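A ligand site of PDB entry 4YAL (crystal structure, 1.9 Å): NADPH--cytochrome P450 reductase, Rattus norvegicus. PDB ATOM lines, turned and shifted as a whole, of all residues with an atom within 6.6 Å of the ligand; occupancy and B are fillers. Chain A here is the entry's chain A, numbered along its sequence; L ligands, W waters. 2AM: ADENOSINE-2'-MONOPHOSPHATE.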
ATOM      1  N   ARG A 242      -1.151 -33.382  13.545  1.00  0.00           N
ATOM      2  CA  ARG A 242      -2.100 -34.438  13.180  1.00  0.00           C
ATOM      3  C   ARG A 242      -1.379 -35.716  12.752  1.00  0.00           C
ATOM      4  O   ARG A 242      -0.175 -35.718  12.488  1.00  0.00           O
ATOM      5  CB  ARG A 242      -2.979 -33.975  12.022  1.00  0.00           C
ATOM      6  CG  ARG A 242      -3.786 -32.704  12.277  1.00  0.00           C
ATOM      7  CD  ARG A 242      -4.300 -32.158  10.952  1.00  0.00           C
ATOM      8  NE  ARG A 242      -3.198 -31.776  10.077  1.00  0.00           N
ATOM      9  CZ  ARG A 242      -3.310 -31.465   8.787  1.00  0.00           C
ATOM     10  NH1 ARG A 242      -4.503 -31.496   8.203  1.00  0.00           N
ATOM     11  NH2 ARG A 242      -2.241 -31.126   8.094  1.00  0.00           N
ATOM     12  N   PRO A 477     -10.026 -32.479  -1.265  1.00  0.00           N
ATOM     13  CA  PRO A 477      -8.927 -31.992  -0.421  1.00  0.00           C
ATOM     14  C   PRO A 477      -8.768 -32.865   0.831  1.00  0.00           C
ATOM     15  O   PRO A 477      -9.681 -33.585   1.217  1.00  0.00           O
ATOM     16  CB  PRO A 477      -9.366 -30.572  -0.089  1.00  0.00           C
ATOM     17  CG  PRO A 477     -10.865 -30.692  -0.024  1.00  0.00           C
ATOM     18  CD  PRO A 477     -11.167 -31.550  -1.246  1.00  0.00           C
ATOM     19  N   GLY A 478      -7.605 -32.780   1.471  1.00  0.00           N
ATOM     20  CA  GLY A 478      -7.362 -33.577   2.663  1.00  0.00           C
ATOM     21  C   GLY A 478      -7.530 -35.055   2.396  1.00  0.00           C
ATOM     22  O   GLY A 478      -7.098 -35.569   1.352  1.00  0.00           O
ATOM     23  N   THR A 479      -8.167 -35.758   3.332  1.00  0.00           N
ATOM     24  CA  THR A 479      -8.402 -37.199   3.178  1.00  0.00           C
ATOM     25  C   THR A 479      -9.428 -37.463   2.093  1.00  0.00           C
ATOM     26  O   THR A 479      -9.731 -38.610   1.772  1.00  0.00           O
ATOM     27  CB  THR A 479      -8.898 -37.828   4.486  1.00  0.00           C
ATOM     28  OG1 THR A 479     -10.080 -37.137   4.927  1.00  0.00           O
ATOM     29  CG2 THR A 479      -7.824 -37.760   5.563  1.00  0.00           C
ATOM     30  N   GLY A 509      -6.219 -30.487  -2.126  1.00  0.00           N
ATOM     31  CA  GLY A 509      -5.867 -29.401  -1.234  1.00  0.00           C
ATOM     32  C   GLY A 509      -5.325 -29.881   0.099  1.00  0.00           C
ATOM     33  O   GLY A 509      -5.727 -30.919   0.604  1.00  0.00           O
ATOM     34  N   CYS A 510      -4.374 -29.124   0.637  1.00  0.00           N
ATOM     35  CA  CYS A 510      -3.767 -29.417   1.938  1.00  0.00           C
ATOM     36  C   CYS A 510      -3.241 -28.092   2.478  1.00  0.00           C
ATOM     37  O   CYS A 510      -3.377 -27.058   1.821  1.00  0.00           O
ATOM     38  CB  CYS A 510      -2.623 -30.434   1.800  1.00  0.00           C
ATOM     39  SG  CYS A 510      -1.214 -29.904   0.805  1.00  0.00           S
ATOM     40  N   ARG A 511      -2.650 -28.102   3.671  1.00  0.00           N
ATOM     41  CA  ARG A 511      -2.158 -26.864   4.265  1.00  0.00           C
ATOM     42  C   ARG A 511      -0.866 -26.356   3.619  1.00  0.00           C
ATOM     43  O   ARG A 511      -0.820 -25.211   3.143  1.00  0.00           O
ATOM     44  CB  ARG A 511      -1.952 -27.044   5.772  1.00  0.00           C
ATOM     45  CG  ARG A 511      -3.224 -27.458   6.504  1.00  0.00           C
ATOM     46  CD  ARG A 511      -2.988 -27.697   7.995  1.00  0.00           C
ATOM     47  NE  ARG A 511      -4.223 -28.118   8.644  1.00  0.00           N
ATOM     48  CZ  ARG A 511      -4.344 -28.365   9.947  1.00  0.00           C
ATOM     49  NH1 ARG A 511      -3.314 -28.226  10.765  1.00  0.00           N
ATOM     50  NH2 ARG A 511      -5.516 -28.753  10.433  1.00  0.00           N
ATOM     51  N   ARG A 512       0.179 -27.178   3.615  1.00  0.00           N
ATOM     52  CA  ARG A 512       1.469 -26.788   3.036  1.00  0.00           C
ATOM     53  C   ARG A 512       2.133 -27.944   2.302  1.00  0.00           C
ATOM     54  O   ARG A 512       2.113 -29.077   2.785  1.00  0.00           O
ATOM     55  CB  ARG A 512       2.409 -26.260   4.123  1.00  0.00           C
ATOM     56  CG  ARG A 512       1.876 -25.053   4.888  1.00  0.00           C
ATOM     57  CD  ARG A 512       3.002 -24.362   5.651  1.00  0.00           C
ATOM     58  NE  ARG A 512       2.539 -23.163   6.350  1.00  0.00           N
ATOM     59  CZ  ARG A 512       1.721 -23.161   7.389  1.00  0.00           C
ATOM     60  NH1 ARG A 512       1.243 -24.303   7.875  1.00  0.00           N
ATOM     61  NH2 ARG A 512       1.361 -22.015   7.964  1.00  0.00           N
ATOM     62  N   ASP A 516       1.812 -31.610   4.672  1.00  0.00           N
ATOM     63  CA  ASP A 516       0.707 -32.572   4.603  1.00  0.00           C
ATOM     64  C   ASP A 516       0.184 -32.824   3.196  1.00  0.00           C
ATOM     65  O   ASP A 516      -1.020 -32.993   2.987  1.00  0.00           O
ATOM     66  CB  ASP A 516      -0.436 -32.060   5.480  1.00  0.00           C
ATOM     67  CG  ASP A 516      -0.980 -30.718   5.001  1.00  0.00           C
ATOM     68  OD1 ASP A 516      -0.223 -29.960   4.350  1.00  0.00           O
ATOM     69  OD2 ASP A 516      -2.150 -30.406   5.300  1.00  0.00           O
ATOM     70  N   ALA A 538      -4.241 -26.860  -4.046  1.00  0.00           N
ATOM     71  CA  ALA A 538      -4.445 -25.640  -3.304  1.00  0.00           C
ATOM     72  C   ALA A 538      -3.782 -25.803  -1.944  1.00  0.00           C
ATOM     73  O   ALA A 538      -4.185 -26.660  -1.160  1.00  0.00           O
ATOM     74  CB  ALA A 538      -5.950 -25.390  -3.137  1.00  0.00           C
ATOM     75  N   PHE A 539      -2.748 -25.007  -1.673  1.00  0.00           N
ATOM     76  CA  PHE A 539      -2.069 -25.046  -0.383  1.00  0.00           C
ATOM     77  C   PHE A 539      -2.719 -23.911   0.393  1.00  0.00           C
ATOM     78  O   PHE A 539      -2.435 -22.736   0.144  1.00  0.00           O
ATOM     79  CB  PHE A 539      -0.563 -24.820  -0.574  1.00  0.00           C
ATOM     80  CG  PHE A 539       0.107 -25.876  -1.413  1.00  0.00           C
ATOM     81  CD1 PHE A 539       0.158 -27.200  -0.982  1.00  0.00           C
ATOM     82  CD2 PHE A 539       0.643 -25.547  -2.654  1.00  0.00           C
ATOM     83  CE1 PHE A 539       0.737 -28.190  -1.781  1.00  0.00           C
ATOM     84  CE2 PHE A 539       1.226 -26.527  -3.455  1.00  0.00           C
ATOM     85  CZ  PHE A 539       1.265 -27.855  -3.012  1.00  0.00           C
ATOM     86  N   SER A 540      -3.591 -24.267   1.324  1.00  0.00           N
ATOM     87  CA  SER A 540      -4.349 -23.288   2.081  1.00  0.00           C
ATOM     88  C   SER A 540      -3.585 -22.361   3.028  1.00  0.00           C
ATOM     89  O   SER A 540      -4.077 -21.276   3.329  1.00  0.00           O
ATOM     90  CB  SER A 540      -5.473 -23.974   2.848  1.00  0.00           C
ATOM     91  OG  SER A 540      -4.972 -24.886   3.808  1.00  0.00           O
ATOM     92  N   ARG A 541      -2.407 -22.774   3.482  1.00  0.00           N
ATOM     93  CA  ARG A 541      -1.650 -21.944   4.422  1.00  0.00           C
ATOM     94  C   ARG A 541      -0.284 -21.457   3.955  1.00  0.00           C
ATOM     95  O   ARG A 541       0.530 -21.000   4.769  1.00  0.00           O
ATOM     96  CB  ARG A 541      -1.518 -22.682   5.759  1.00  0.00           C
ATOM     97  CG  ARG A 541      -2.851 -23.172   6.285  1.00  0.00           C
ATOM     98  CD  ARG A 541      -2.786 -23.737   7.705  1.00  0.00           C
ATOM     99  NE  ARG A 541      -4.094 -24.262   8.091  1.00  0.00           N
ATOM    100  CZ  ARG A 541      -4.380 -24.766   9.292  1.00  0.00           C
ATOM    101  NH1 ARG A 541      -3.456 -24.814  10.237  1.00  0.00           N
ATOM    102  NH2 ARG A 541      -5.603 -25.230   9.541  1.00  0.00           N
ATOM    103  N   LYS A 546      -6.637 -17.779   2.325  1.00  0.00           N
ATOM    104  CA  LYS A 546      -6.926 -19.187   2.110  1.00  0.00           C
ATOM    105  C   LYS A 546      -7.042 -19.468   0.619  1.00  0.00           C
ATOM    106  O   LYS A 546      -7.636 -18.697  -0.112  1.00  0.00           O
ATOM    107  CB  LYS A 546      -8.246 -19.581   2.784  1.00  0.00           C
ATOM    108  CG  LYS A 546      -8.249 -19.511   4.295  1.00  0.00           C
ATOM    109  CD  LYS A 546      -7.266 -20.508   4.888  1.00  0.00           C
ATOM    110  CE  LYS A 546      -7.319 -20.505   6.403  1.00  0.00           C
ATOM    111  NZ  LYS A 546      -6.331 -21.464   6.981  1.00  0.00           N
ATOM    112  N   VAL A 547      -6.441 -20.568   0.177  1.00  0.00           N
ATOM    113  CA  VAL A 547      -6.552 -20.975  -1.216  1.00  0.00           C
ATOM    114  C   VAL A 547      -7.116 -22.374  -1.083  1.00  0.00           C
ATOM    115  O   VAL A 547      -6.456 -23.257  -0.526  1.00  0.00           O
ATOM    116  CB  VAL A 547      -5.190 -21.000  -1.927  1.00  0.00           C
ATOM    117  CG1 VAL A 547      -5.360 -21.574  -3.343  1.00  0.00           C
ATOM    118  CG2 VAL A 547      -4.621 -19.595  -2.012  1.00  0.00           C
ATOM    119  N   TYR A 548      -8.338 -22.561  -1.562  1.00  0.00           N
ATOM    120  CA  TYR A 548      -9.024 -23.855  -1.492  1.00  0.00           C
ATOM    121  C   TYR A 548      -9.292 -24.408  -2.891  1.00  0.00           C
ATOM    122  O   TYR A 548      -9.133 -23.704  -3.875  1.00  0.00           O
ATOM    123  CB  TYR A 548     -10.349 -23.720  -0.749  1.00  0.00           C
ATOM    124  CG  TYR A 548     -10.263 -23.324   0.709  1.00  0.00           C
ATOM    125  CD1 TYR A 548      -9.268 -23.845   1.550  1.00  0.00           C
ATOM    126  CD2 TYR A 548     -11.228 -22.489   1.282  1.00  0.00           C
ATOM    127  CE1 TYR A 548      -9.242 -23.560   2.918  1.00  0.00           C
ATOM    128  CE2 TYR A 548     -11.212 -22.201   2.650  1.00  0.00           C
ATOM    129  CZ  TYR A 548     -10.224 -22.737   3.453  1.00  0.00           C
ATOM    130  OH  TYR A 548     -10.243 -22.480   4.808  1.00  0.00           O
ATOM    131  N   VAL A 549      -9.716 -25.659  -2.963  1.00  0.00           N
ATOM    132  CA  VAL A 549      -9.987 -26.278  -4.252  1.00  0.00           C
ATOM    133  C   VAL A 549     -11.006 -25.505  -5.085  1.00  0.00           C
ATOM    134  O   VAL A 549     -10.857 -25.406  -6.298  1.00  0.00           O
ATOM    135  CB  VAL A 549     -10.441 -27.751  -4.098  1.00  0.00           C
ATOM    136  CG1 VAL A 549      -9.298 -28.594  -3.561  1.00  0.00           C
ATOM    137  CG2 VAL A 549     -11.645 -27.862  -3.170  1.00  0.00           C
ATOM    138  N   GLN A 550     -12.042 -24.949  -4.457  1.00  0.00           N
ATOM    139  CA  GLN A 550     -13.052 -24.210  -5.215  1.00  0.00           C
ATOM    140  C   GLN A 550     -12.484 -22.964  -5.896  1.00  0.00           C
ATOM    141  O   GLN A 550     -13.028 -22.492  -6.903  1.00  0.00           O
ATOM    142  CB  GLN A 550     -14.241 -23.809  -4.328  1.00  0.00           C
ATOM    143  CG  GLN A 550     -13.857 -23.016  -3.095  1.00  0.00           C
ATOM    144  CD  GLN A 550     -13.697 -23.885  -1.875  1.00  0.00           C
ATOM    145  OE1 GLN A 550     -13.219 -25.024  -1.955  1.00  0.00           O
ATOM    146  NE2 GLN A 550     -14.077 -23.362  -0.715  1.00  0.00           N
ATOM    147  N   ASP A 576     -14.879 -33.554   3.318  1.00  0.00           N
ATOM    148  CA  ASP A 576     -15.715 -32.829   4.259  1.00  0.00           C
ATOM    149  C   ASP A 576     -17.074 -32.428   3.691  1.00  0.00           C
ATOM    150  O   ASP A 576     -17.169 -31.685   2.716  1.00  0.00           O
ATOM    151  CB  ASP A 576     -14.996 -31.582   4.740  1.00  0.00           C
ATOM    152  CG  ASP A 576     -15.905 -30.685   5.552  1.00  0.00           C
ATOM    153  OD1 ASP A 576     -16.492 -31.191   6.538  1.00  0.00           O
ATOM    154  OD2 ASP A 576     -16.038 -29.487   5.207  1.00  0.00           O
ATOM    155  N   ASN A 579     -18.597 -28.017   5.070  1.00  0.00           N
ATOM    156  CA  ASN A 579     -18.450 -26.763   4.326  1.00  0.00           C
ATOM    157  C   ASN A 579     -17.858 -26.913   2.923  1.00  0.00           C
ATOM    158  O   ASN A 579     -18.326 -26.262   1.985  1.00  0.00           O
ATOM    159  CB  ASN A 579     -17.592 -25.782   5.115  1.00  0.00           C
ATOM    160  CG  ASN A 579     -18.296 -25.264   6.366  1.00  0.00           C
ATOM    161  OD1 ASN A 579     -18.589 -26.022   7.288  1.00  0.00           O
ATOM    162  ND2 ASN A 579     -18.578 -23.961   6.395  1.00  0.00           N
ATOM    163  N   MET A 580     -16.838 -27.759   2.783  1.00  0.00           N
ATOM    164  CA  MET A 580     -16.202 -27.941   1.481  1.00  0.00           C
ATOM    165  C   MET A 580     -17.153 -28.391   0.385  1.00  0.00           C
ATOM    166  O   MET A 580     -17.195 -27.797  -0.696  1.00  0.00           O
ATOM    167  CB  MET A 580     -15.036 -28.929   1.621  1.00  0.00           C
ATOM    168  CG  MET A 580     -14.220 -29.149   0.338  1.00  0.00           C
ATOM    169  SD  MET A 580     -14.981 -30.282  -0.844  1.00  0.00           S
ATOM    170  CE  MET A 580     -14.862 -31.850   0.101  1.00  0.00           C
ATOM    171  N   ALA A 581     -17.945 -29.434   0.643  1.00  0.00           N
ATOM    172  CA  ALA A 581     -18.878 -29.950  -0.355  1.00  0.00           C
ATOM    173  C   ALA A 581     -19.805 -28.873  -0.924  1.00  0.00           C
ATOM    174  O   ALA A 581     -19.964 -28.759  -2.142  1.00  0.00           O
ATOM    175  CB  ALA A 581     -19.705 -31.083   0.243  1.00  0.00           C
ATOM    176  N   ASP A 583     -19.446 -25.523  -0.649  1.00  0.00           N
ATOM    177  CA  ASP A 583     -18.698 -24.451  -1.281  1.00  0.00           C
ATOM    178  C   ASP A 583     -18.339 -24.847  -2.700  1.00  0.00           C
ATOM    179  O   ASP A 583     -18.380 -24.029  -3.620  1.00  0.00           O
ATOM    180  CB  ASP A 583     -17.414 -24.139  -0.501  1.00  0.00           C
ATOM    181  CG  ASP A 583     -17.694 -23.412   0.804  1.00  0.00           C
ATOM    182  OD1 ASP A 583     -18.761 -22.781   0.917  1.00  0.00           O
ATOM    183  OD2 ASP A 583     -16.828 -23.465   1.704  1.00  0.00           O
ATOM    184  N   VAL A 584     -17.959 -26.108  -2.886  1.00  0.00           N
ATOM    185  CA  VAL A 584     -17.603 -26.597  -4.220  1.00  0.00           C
ATOM    186  C   VAL A 584     -18.859 -26.599  -5.096  1.00  0.00           C
ATOM    187  O   VAL A 584     -18.832 -26.122  -6.239  1.00  0.00           O
ATOM    188  CB  VAL A 584     -16.999 -28.021  -4.130  1.00  0.00           C
ATOM    189  CG1 VAL A 584     -16.896 -28.646  -5.514  1.00  0.00           C
ATOM    190  CG2 VAL A 584     -15.620 -27.938  -3.500  1.00  0.00           C
HETATM  191  P   2AM L   1      -7.432 -24.913   6.220  1.00  0.00           P
HETATM  192  O1P 2AM L   1      -8.637 -24.066   6.307  1.00  0.00           O
HETATM  193  O2P 2AM L   1      -7.407 -26.033   7.193  1.00  0.00           O
HETATM  194  O3P 2AM L   1      -6.160 -24.160   6.110  1.00  0.00           O
HETATM  195  C5' 2AM L   1      -7.880 -30.270   4.334  1.00  0.00           C
HETATM  196  O5' 2AM L   1      -8.458 -29.943   5.599  1.00  0.00           O
HETATM  197  C4' 2AM L   1      -7.824 -29.014   3.456  1.00  0.00           C
HETATM  198  O4' 2AM L   1      -9.149 -28.485   3.263  1.00  0.00           O
HETATM  199  C3' 2AM L   1      -7.022 -27.926   4.164  1.00  0.00           C
HETATM  200  O3' 2AM L   1      -6.157 -27.274   3.224  1.00  0.00           O
HETATM  201  C2' 2AM L   1      -8.102 -26.965   4.629  1.00  0.00           C
HETATM  202  O2' 2AM L   1      -7.567 -25.636   4.781  1.00  0.00           O
HETATM  203  C1' 2AM L   1      -9.054 -27.069   3.444  1.00  0.00           C
HETATM  204  N9  2AM L   1     -10.379 -26.472   3.698  1.00  0.00           N
HETATM  205  C8  2AM L   1     -10.880 -26.084   4.867  1.00  0.00           C
HETATM  206  N7  2AM L   1     -12.119 -25.658   4.660  1.00  0.00           N
HETATM  207  C5  2AM L   1     -12.395 -25.794   3.366  1.00  0.00           C
HETATM  208  C6  2AM L   1     -13.473 -25.458   2.650  1.00  0.00           C
HETATM  209  N6  2AM L   1     -14.514 -24.970   3.318  1.00  0.00           N
HETATM  210  N1  2AM L   1     -13.520 -25.639   1.321  1.00  0.00           N
HETATM  211  C2  2AM L   1     -12.422 -26.201   0.678  1.00  0.00           C
HETATM  212  N3  2AM L   1     -11.301 -26.544   1.452  1.00  0.00           N
HETATM  213  C4  2AM L   1     -11.322 -26.315   2.771  1.00  0.00           C
HETATM  214  O   HOH W   1      -9.250 -27.123  -0.494  1.00  0.00           O
HETATM  215  O   HOH W   2      -6.626 -26.473   0.521  1.00  0.00           O
HETATM  216  O   HOH W   3      -4.707 -31.247   5.035  1.00  0.00           O
HETATM  217  O   HOH W   4      -6.673 -28.549   7.533  1.00  0.00           O
HETATM  218  O   HOH W   5      -9.817 -23.089   8.623  1.00  0.00           O
HETATM  219  O   HOH W   6     -13.996 -25.161   6.986  1.00  0.00           O
HETATM  220  O   HOH W   7     -11.932 -29.859   3.174  1.00  0.00           O
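The side-chain hydroxyl (OG) of Ser 540 lies within hydrogen-bond range of an oxygen (O3P) of the ligand (2.7 Å). OH of Tyr 548 lies within hydrogen-bond range of O1P of the ligand (2.7 Å). The side-chain amino group (NZ) of Lys 546 is in salt-bridge range of an oxygen (O3P) of the ligand (2.8 Å). O3P of the ligand is in salt-bridge range of NE of Arg 541 (2.9 Å). The side-chain amide nitrogen (NE2) of Gln 550 is in hydrogen-bond range of a nitrogen (N1) of the ligand, at 3.1 Å. The backbone carbonyl oxygen (O) of Cys 510 lies close to an oxygen (O3') of the ligand, 3.1 Å away. N6 of the ligand sits at hydrogen-bond distance from OD2 of Asp 583 (3.2 Å).
Residues that only touch the ligand: Pro 477 (3.95 Å), Gly 478 (3.7 Å), Arg 511 (3.6 Å), Asn 579 (3.7 Å) and Met 580 (3.5 Å). Hydrophobic or aromatic side chains that line the ligand: Pro 477, Tyr 548 and Met 580. 12 residues have an atom within 4 Å of the ligand: Pro 477, Gly 478, Cys 510, Arg 511, Ser 540, Arg 541, Lys 546, Tyr 548, Gln 550, Asn 579, Met 580 and Asp 583. Along chain A the residues within 4 Å of the ligand span positions 477 to 583.
Water W4 bridges an oxygen (O2P) of the ligand (2.6 Å) and the guanidinium group (NE) of Arg 511 (2.7 Å). Water W2 lies within hydrogen-bond range of O3' of the ligand (2.9 Å), O of Ala 538 (3.0 Å), O of Val 547 (3.4 Å) and N of Cys 510 (3.5 Å). Water W1 bridges a nitrogen (N3) of the ligand and the backbone NH (N) of Val 549. Water W3 lies within hydrogen-bond range of OD2 of Asp 516 (2.7 Å) and NH1 of Arg 242 (3.2 Å).
The backbone NH (N) of Ser 540 lies within hydrogen-bond range of the backbone carbonyl oxygen (O) of Cys 510, 2.8 Å away. The backbone NH (N) of Ser 540 lies within hydrogen-bond range of the backbone carbonyl oxygen (O) of Arg 511 (3.4 Å). The backbone NH (N) of Arg 541 sits at hydrogen-bond distance from the backbone carbonyl oxygen (O) of Arg 511 (2.9 Å). O of Arg 541 is in hydrogen-bond range of NE of Arg 512 (3.3 Å). N of Cys 510 is in hydrogen-bond range of O of Ala 538, 3.1 Å away. The side-chain sulfur (SG) of Cys 510 lies close to the side-chain carboxylate (OD1) of Asp 516, 3.7 Å away. The side-chain carboxylate (OD2) of Asp 516 is in hydrogen-bond range of the backbone NH (N) of Arg 511, at 2.9 Å. OD2 of Asp 576 lies within hydrogen-bond range of N of Asn 579 (3.0 Å).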
